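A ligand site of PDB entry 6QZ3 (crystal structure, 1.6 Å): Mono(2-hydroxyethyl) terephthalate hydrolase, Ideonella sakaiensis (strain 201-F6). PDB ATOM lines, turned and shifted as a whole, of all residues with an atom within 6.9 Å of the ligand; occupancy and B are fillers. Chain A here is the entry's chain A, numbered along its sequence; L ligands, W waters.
The backbone NH (N) of Arg 411 sits at hydrogen-bond distance from the backbone carbonyl oxygen (O) of Trp 397, 3.0 Å away.
N of Gln 410 is in hydrogen-bond range of O of Trp 397 (3.3 Å).
The guanidinium group (NH2) of Arg 411 sits at hydrogen-bond distance from the backbone carbonyl oxygen (O) of Ala 494 (2.8 Å).
The backbone NH of Ser 416 is in hydrogen-bond range of the backbone carbonyl oxygen of Gln 410 (3.2 Å).
O of Ala 249 sits close to N of Ser 225 (3.4 Å).
OG of Ser 225 is in hydrogen-bond range of NE2 of His 528 (2.6 Å).
The backbone carbonyl oxygen (O) of Ser 225 sits at hydrogen-bond distance from the backbone NH (N) of Gly 251.
OG of Ser 416 sits at hydrogen-bond distance from NE of Arg 411 (2.7 Å).
O of Gly 132 touches C6 of the ligand, at 3.4 Å.
Ser 225 touches the ligand (OG to C5, 3.0 Å).
CD2 of Leu 254 touches C7 of the ligand, 3.6 Å away.
Ala 257 touches the ligand (CB to O1, 3.7 Å).
CH2 of Trp 397 touches C4 of the ligand, 3.6 Å away.
Phe 415 touches the ligand (CE1 to C7, 3.5 Å).
Phe 495 touches the ligand.
NE2 of His 528 touches C4 of the ligand (3.8 Å).
Hydrophobic or aromatic side chains within 4 Å of the ligand: Leu 254, Ala 257, Trp 397, Phe 415 and Phe 495.
Of the 24 residues printed, 10 come within 4 Å of the ligand.
O1 of the ligand lies within hydrogen-bond range of OG of Ser 416, 2.6 Å away.
NH2 of Arg 411 is in salt-bridge range of O1 of the ligand (2.9 Å).
Water W1 lies within hydrogen-bond range of O2 of the ligand (2.6 Å) and O of Ser 416 (2.8 Å).
Water W2 bridges the side-chain hydroxyl of Ser 419 (2.8 Å) and an oxygen (O2) of the ligand (2.8 Å).
Water W3 bridges the side-chain hydroxyl of Ser 225 (2.8 Å) and the backbone NH of Gly 132 (2.9 Å).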
ATOM      1  N   SER A 131      25.457  -2.613  12.360  1.00  0.00           N
ATOM      2  CA  SER A 131      25.440  -3.116  13.721  1.00  0.00           C
ATOM      3  C   SER A 131      24.743  -2.101  14.616  1.00  0.00           C
ATOM      4  O   SER A 131      24.792  -0.896  14.348  1.00  0.00           O
ATOM      5  CB  SER A 131      26.864  -3.378  14.237  1.00  0.00           C
ATOM      6  OG  SER A 131      27.588  -2.168  14.333  1.00  0.00           O
ATOM      7  N   GLY A 132      24.097  -2.589  15.662  1.00  0.00           N
ATOM      8  CA  GLY A 132      23.409  -1.704  16.580  1.00  0.00           C
ATOM      9  C   GLY A 132      22.320  -0.916  15.866  1.00  0.00           C
ATOM     10  O   GLY A 132      21.526  -1.469  15.104  1.00  0.00           O
ATOM     11  N   THR A 133      22.294   0.388  16.122  1.00  0.00           N
ATOM     12  CA  THR A 133      21.411   1.300  15.419  1.00  0.00           C
ATOM     13  C   THR A 133      22.132   2.029  14.288  1.00  0.00           C
ATOM     14  O   THR A 133      21.679   3.098  13.857  1.00  0.00           O
ATOM     15  CB  THR A 133      20.791   2.302  16.387  1.00  0.00           C
ATOM     16  OG1 THR A 133      21.825   3.001  17.090  1.00  0.00           O
ATOM     17  CG2 THR A 133      19.890   1.581  17.391  1.00  0.00           C
ATOM     18  N   CYS A 224      25.909  -9.283  10.198  1.00  0.00           N
ATOM     19  CA  CYS A 224      25.479  -9.933  11.429  1.00  0.00           C
ATOM     20  C   CYS A 224      24.699  -8.936  12.267  1.00  0.00           C
ATOM     21  O   CYS A 224      24.959  -7.733  12.204  1.00  0.00           O
ATOM     22  CB  CYS A 224      26.667 -10.502  12.245  1.00  0.00           C
ATOM     23  SG  CYS A 224      26.231 -11.755  13.508  1.00  0.00           S
ATOM     24  N   SER A 225      23.736  -9.440  13.041  1.00  0.00           N
ATOM     25  CA  SER A 225      22.951  -8.627  13.967  1.00  0.00           C
ATOM     26  C   SER A 225      22.018  -7.708  13.188  1.00  0.00           C
ATOM     27  O   SER A 225      21.188  -8.184  12.408  1.00  0.00           O
ATOM     28  CB  SER A 225      23.870  -7.839  14.902  1.00  0.00           C
ATOM     29  OG  SER A 225      23.158  -7.242  15.956  1.00  0.00           O
ATOM     30  N   GLU A 226      22.114  -6.393  13.395  1.00  0.00           N
ATOM     31  CA  GLU A 226      21.411  -5.467  12.509  1.00  0.00           C
ATOM     32  C   GLU A 226      21.817  -5.693  11.052  1.00  0.00           C
ATOM     33  O   GLU A 226      20.986  -5.554  10.142  1.00  0.00           O
ATOM     34  CB  GLU A 226      21.670  -4.018  12.934  1.00  0.00           C
ATOM     35  CG  GLU A 226      21.568  -2.979  11.815  1.00  0.00           C
ATOM     36  CD  GLU A 226      20.155  -2.811  11.266  1.00  0.00           C
ATOM     37  OE1 GLU A 226      19.185  -3.131  11.984  1.00  0.00           O
ATOM     38  OE2 GLU A 226      20.005  -2.364  10.112  1.00  0.00           O
ATOM     39  N   ALA A 249      22.890 -13.916  13.068  1.00  0.00           N
ATOM     40  CA  ALA A 249      22.067 -13.484  14.198  1.00  0.00           C
ATOM     41  C   ALA A 249      21.087 -12.397  13.779  1.00  0.00           C
ATOM     42  O   ALA A 249      21.128 -11.283  14.328  1.00  0.00           O
ATOM     43  CB  ALA A 249      22.951 -13.005  15.349  1.00  0.00           C
ATOM     44  N   GLY A 251      18.327  -9.724  13.188  1.00  0.00           N
ATOM     45  CA  GLY A 251      17.238  -9.083  13.901  1.00  0.00           C
ATOM     46  C   GLY A 251      16.070  -8.794  12.985  1.00  0.00           C
ATOM     47  O   GLY A 251      15.646  -7.642  12.856  1.00  0.00           O
ATOM     48  N   LEU A 254      13.280  -6.899  14.650  1.00  0.00           N
ATOM     49  CA  LEU A 254      13.891  -6.011  15.632  1.00  0.00           C
ATOM     50  C   LEU A 254      12.915  -5.152  16.436  1.00  0.00           C
ATOM     51  O   LEU A 254      13.147  -4.988  17.644  1.00  0.00           O
ATOM     52  CB  LEU A 254      14.925  -5.106  14.915  1.00  0.00           C
ATOM     53  CG  LEU A 254      16.364  -5.469  15.245  1.00  0.00           C
ATOM     54  CD1 LEU A 254      17.344  -4.780  14.291  1.00  0.00           C
ATOM     55  CD2 LEU A 254      16.650  -5.087  16.680  1.00  0.00           C
ATOM     56  N   ALA A 257      12.144  -6.532  19.852  1.00  0.00           N
ATOM     57  CA  ALA A 257      13.175  -6.769  20.866  1.00  0.00           C
ATOM     58  C   ALA A 257      12.876  -6.007  22.152  1.00  0.00           C
ATOM     59  O   ALA A 257      13.057  -6.544  23.251  1.00  0.00           O
ATOM     60  CB  ALA A 257      14.550  -6.385  20.317  1.00  0.00           C
ATOM     61  N   GLY A 258      12.427  -4.756  22.038  1.00  0.00           N
ATOM     62  CA  GLY A 258      12.112  -3.986  23.226  1.00  0.00           C
ATOM     63  C   GLY A 258      10.919  -4.535  23.992  1.00  0.00           C
ATOM     64  O   GLY A 258      10.805  -4.322  25.202  1.00  0.00           O
ATOM     65  N   TRP A 397      22.874  -8.526  28.077  1.00  0.00           N
ATOM     66  CA  TRP A 397      21.707  -8.067  27.345  1.00  0.00           C
ATOM     67  C   TRP A 397      20.518  -7.821  28.256  1.00  0.00           C
ATOM     68  O   TRP A 397      19.922  -6.732  28.223  1.00  0.00           O
ATOM     69  CB  TRP A 397      21.360  -9.080  26.246  1.00  0.00           C
ATOM     70  CG  TRP A 397      22.344  -8.990  25.132  1.00  0.00           C
ATOM     71  CD1 TRP A 397      23.448  -9.776  24.955  1.00  0.00           C
ATOM     72  CD2 TRP A 397      22.352  -8.036  24.074  1.00  0.00           C
ATOM     73  NE1 TRP A 397      24.131  -9.368  23.824  1.00  0.00           N
ATOM     74  CE2 TRP A 397      23.482  -8.303  23.276  1.00  0.00           C
ATOM     75  CE3 TRP A 397      21.504  -6.973  23.712  1.00  0.00           C
ATOM     76  CZ2 TRP A 397      23.784  -7.559  22.138  1.00  0.00           C
ATOM     77  CZ3 TRP A 397      21.811  -6.238  22.583  1.00  0.00           C
ATOM     78  CH2 TRP A 397      22.932  -6.529  21.813  1.00  0.00           C
ATOM     79  N   GLN A 410      21.426  -3.809  28.255  1.00  0.00           N
ATOM     80  CA  GLN A 410      20.954  -3.179  27.028  1.00  0.00           C
ATOM     81  C   GLN A 410      19.427  -3.080  27.005  1.00  0.00           C
ATOM     82  O   GLN A 410      18.877  -2.120  26.455  1.00  0.00           O
ATOM     83  CB  GLN A 410      21.455  -3.947  25.806  1.00  0.00           C
ATOM     84  CG  GLN A 410      22.873  -4.463  25.925  1.00  0.00           C
ATOM     85  CD  GLN A 410      23.888  -3.346  26.017  1.00  0.00           C
ATOM     86  OE1 GLN A 410      23.678  -2.251  25.480  1.00  0.00           O
ATOM     87  NE2 GLN A 410      25.003  -3.602  26.698  1.00  0.00           N
ATOM     88  N   ARG A 411      18.734  -4.060  27.584  1.00  0.00           N
ATOM     89  CA  ARG A 411      17.288  -4.131  27.532  1.00  0.00           C
ATOM     90  C   ARG A 411      16.599  -3.419  28.689  1.00  0.00           C
ATOM     91  O   ARG A 411      15.374  -3.276  28.659  1.00  0.00           O
ATOM     92  CB  ARG A 411      16.834  -5.591  27.504  1.00  0.00           C
ATOM     93  CG  ARG A 411      17.212  -6.329  26.224  1.00  0.00           C
ATOM     94  CD  ARG A 411      16.188  -6.082  25.110  1.00  0.00           C
ATOM     95  NE  ARG A 411      16.776  -6.206  23.775  1.00  0.00           N
ATOM     96  CZ  ARG A 411      17.042  -7.361  23.177  1.00  0.00           C
ATOM     97  NH1 ARG A 411      16.779  -8.508  23.783  1.00  0.00           N
ATOM     98  NH2 ARG A 411      17.563  -7.357  21.955  1.00  0.00           N
ATOM     99  N   PHE A 415      20.839   0.799  25.025  1.00  0.00           N
ATOM    100  CA  PHE A 415      20.458   1.300  23.704  1.00  0.00           C
ATOM    101  C   PHE A 415      19.248   0.563  23.141  1.00  0.00           C
ATOM    102  O   PHE A 415      18.532   1.127  22.309  1.00  0.00           O
ATOM    103  CB  PHE A 415      21.642   1.213  22.744  1.00  0.00           C
ATOM    104  CG  PHE A 415      21.762  -0.104  22.024  1.00  0.00           C
ATOM    105  CD1 PHE A 415      21.162  -0.299  20.789  1.00  0.00           C
ATOM    106  CD2 PHE A 415      22.490  -1.145  22.580  1.00  0.00           C
ATOM    107  CE1 PHE A 415      21.262  -1.509  20.136  1.00  0.00           C
ATOM    108  CE2 PHE A 415      22.604  -2.358  21.925  1.00  0.00           C
ATOM    109  CZ  PHE A 415      21.986  -2.543  20.703  1.00  0.00           C
ATOM    110  N   SER A 416      19.022  -0.681  23.550  1.00  0.00           N
ATOM    111  CA  SER A 416      17.885  -1.423  23.001  1.00  0.00           C
ATOM    112  C   SER A 416      16.568  -0.849  23.499  1.00  0.00           C
ATOM    113  O   SER A 416      15.636  -0.640  22.717  1.00  0.00           O
ATOM    114  CB  SER A 416      17.994  -2.907  23.372  1.00  0.00           C
ATOM    115  OG  SER A 416      16.880  -3.630  22.864  1.00  0.00           O
ATOM    116  N   ALA A 417      16.483  -0.589  24.805  1.00  0.00           N
ATOM    117  CA  ALA A 417      15.289   0.054  25.344  1.00  0.00           C
ATOM    118  C   ALA A 417      15.107   1.447  24.763  1.00  0.00           C
ATOM    119  O   ALA A 417      13.987   1.844  24.405  1.00  0.00           O
ATOM    120  CB  ALA A 417      15.384   0.112  26.872  1.00  0.00           C
ATOM    121  N   SER A 419      16.211   2.565  21.834  1.00  0.00           N
ATOM    122  CA  SER A 419      15.849   2.462  20.432  1.00  0.00           C
ATOM    123  C   SER A 419      14.375   2.112  20.253  1.00  0.00           C
ATOM    124  O   SER A 419      13.718   2.620  19.338  1.00  0.00           O
ATOM    125  CB  SER A 419      16.730   1.432  19.723  1.00  0.00           C
ATOM    126  OG  SER A 419      16.400   1.333  18.349  1.00  0.00           O
ATOM    127  N   TRP A 420      13.834   1.245  21.120  1.00  0.00           N
ATOM    128  CA  TRP A 420      12.416   0.920  20.991  1.00  0.00           C
ATOM    129  C   TRP A 420      11.550   2.159  21.180  1.00  0.00           C
ATOM    130  O   TRP A 420      10.600   2.376  20.421  1.00  0.00           O
ATOM    131  CB  TRP A 420      12.014  -0.158  21.991  1.00  0.00           C
ATOM    132  CG  TRP A 420      10.640  -0.687  21.691  1.00  0.00           C
ATOM    133  CD1 TRP A 420      10.326  -1.718  20.869  1.00  0.00           C
ATOM    134  CD2 TRP A 420       9.399  -0.160  22.188  1.00  0.00           C
ATOM    135  NE1 TRP A 420       8.961  -1.882  20.819  1.00  0.00           N
ATOM    136  CE2 TRP A 420       8.368  -0.942  21.625  1.00  0.00           C
ATOM    137  CE3 TRP A 420       9.048   0.883  23.050  1.00  0.00           C
ATOM    138  CZ2 TRP A 420       7.020  -0.714  21.898  1.00  0.00           C
ATOM    139  CZ3 TRP A 420       7.713   1.106  23.322  1.00  0.00           C
ATOM    140  CH2 TRP A 420       6.714   0.312  22.745  1.00  0.00           C
ATOM    141  N   PHE A 424      11.156   2.668  17.241  1.00  0.00           N
ATOM    142  CA  PHE A 424      10.203   1.644  16.843  1.00  0.00           C
ATOM    143  C   PHE A 424       8.776   1.919  17.311  1.00  0.00           C
ATOM    144  O   PHE A 424       7.835   1.549  16.614  1.00  0.00           O
ATOM    145  CB  PHE A 424      10.656   0.268  17.335  1.00  0.00           C
ATOM    146  CG  PHE A 424      12.009  -0.136  16.805  1.00  0.00           C
ATOM    147  CD1 PHE A 424      12.376   0.177  15.514  1.00  0.00           C
ATOM    148  CD2 PHE A 424      12.918  -0.804  17.619  1.00  0.00           C
ATOM    149  CE1 PHE A 424      13.614  -0.173  15.021  1.00  0.00           C
ATOM    150  CE2 PHE A 424      14.162  -1.165  17.134  1.00  0.00           C
ATOM    151  CZ  PHE A 424      14.513  -0.845  15.825  1.00  0.00           C
ATOM    152  N   HIS A 467      11.331  -1.711   9.142  1.00  0.00           N
ATOM    153  CA  HIS A 467      12.455  -2.441   9.719  1.00  0.00           C
ATOM    154  C   HIS A 467      12.280  -3.955   9.683  1.00  0.00           C
ATOM    155  O   HIS A 467      13.268  -4.685   9.593  1.00  0.00           O
ATOM    156  CB  HIS A 467      12.696  -2.006  11.165  1.00  0.00           C
ATOM    157  CG  HIS A 467      14.139  -2.010  11.561  1.00  0.00           C
ATOM    158  ND1 HIS A 467      15.144  -1.499  10.755  1.00  0.00           N
ATOM    159  CD2 HIS A 467      14.764  -2.467  12.678  1.00  0.00           C
ATOM    160  CE1 HIS A 467      16.310  -1.628  11.368  1.00  0.00           C
ATOM    161  NE2 HIS A 467      16.099  -2.215  12.530  1.00  0.00           N
ATOM    162  N   ALA A 494      20.318 -11.246  22.365  1.00  0.00           N
ATOM    163  CA  ALA A 494      19.760 -10.117  21.636  1.00  0.00           C
ATOM    164  C   ALA A 494      18.550 -10.546  20.810  1.00  0.00           C
ATOM    165  O   ALA A 494      17.481  -9.950  20.909  1.00  0.00           O
ATOM    166  CB  ALA A 494      20.830  -9.500  20.727  1.00  0.00           C
ATOM    167  N   PHE A 495      18.724 -11.587  19.992  1.00  0.00           N
ATOM    168  CA  PHE A 495      17.670 -12.157  19.166  1.00  0.00           C
ATOM    169  C   PHE A 495      17.655 -13.665  19.382  1.00  0.00           C
ATOM    170  O   PHE A 495      18.719 -14.293  19.512  1.00  0.00           O
ATOM    171  CB  PHE A 495      17.880 -11.833  17.676  1.00  0.00           C
ATOM    172  CG  PHE A 495      18.192 -10.387  17.429  1.00  0.00           C
ATOM    173  CD1 PHE A 495      17.327  -9.400  17.837  1.00  0.00           C
ATOM    174  CD2 PHE A 495      19.373 -10.013  16.803  1.00  0.00           C
ATOM    175  CE1 PHE A 495      17.610  -8.062  17.629  1.00  0.00           C
ATOM    176  CE2 PHE A 495      19.661  -8.681  16.584  1.00  0.00           C
ATOM    177  CZ  PHE A 495      18.780  -7.706  17.002  1.00  0.00           C
ATOM    178  N   HIS A 528      25.906 -13.405  21.031  1.00  0.00           N
ATOM    179  CA  HIS A 528      25.438 -12.591  19.910  1.00  0.00           C
ATOM    180  C   HIS A 528      26.602 -12.300  18.961  1.00  0.00           C
ATOM    181  O   HIS A 528      27.486 -11.506  19.283  1.00  0.00           O
ATOM    182  CB  HIS A 528      24.803 -11.292  20.423  1.00  0.00           C
ATOM    183  CG  HIS A 528      24.173 -10.463  19.336  1.00  0.00           C
ATOM    184  ND1 HIS A 528      23.259 -10.972  18.448  1.00  0.00           N
ATOM    185  CD2 HIS A 528      24.340  -9.163  19.011  1.00  0.00           C
ATOM    186  CE1 HIS A 528      22.881 -10.022  17.611  1.00  0.00           C
ATOM    187  NE2 HIS A 528      23.525  -8.913  17.932  1.00  0.00           N
HETATM  188  C1  LIG L   1      18.245  -3.989  19.801  1.00  0.00           C
HETATM  189  O1  LIG L   1      17.815  -4.694  20.741  1.00  0.00           O
HETATM  190  O2  LIG L   1      17.698  -2.902  19.541  1.00  0.00           O
HETATM  191  C2  LIG L   1      19.437  -4.433  19.005  1.00  0.00           C
HETATM  192  C3  LIG L   1      20.166  -5.532  19.422  1.00  0.00           C
HETATM  193  C4  LIG L   1      21.272  -5.933  18.689  1.00  0.00           C
HETATM  194  C5  LIG L   1      21.627  -5.237  17.540  1.00  0.00           C
HETATM  195  C6  LIG L   1      20.889  -4.143  17.124  1.00  0.00           C
HETATM  196  C7  LIG L   1      19.792  -3.739  17.867  1.00  0.00           C
HETATM  197  O   HOH W   1      15.380  -1.997  20.331  1.00  0.00           O
HETATM  198  O   HOH W   2      17.602  -1.040  17.428  1.00  0.00           O
HETATM  199  O   HOH W   3      24.957  -5.189  16.628  1.00  0.00           O
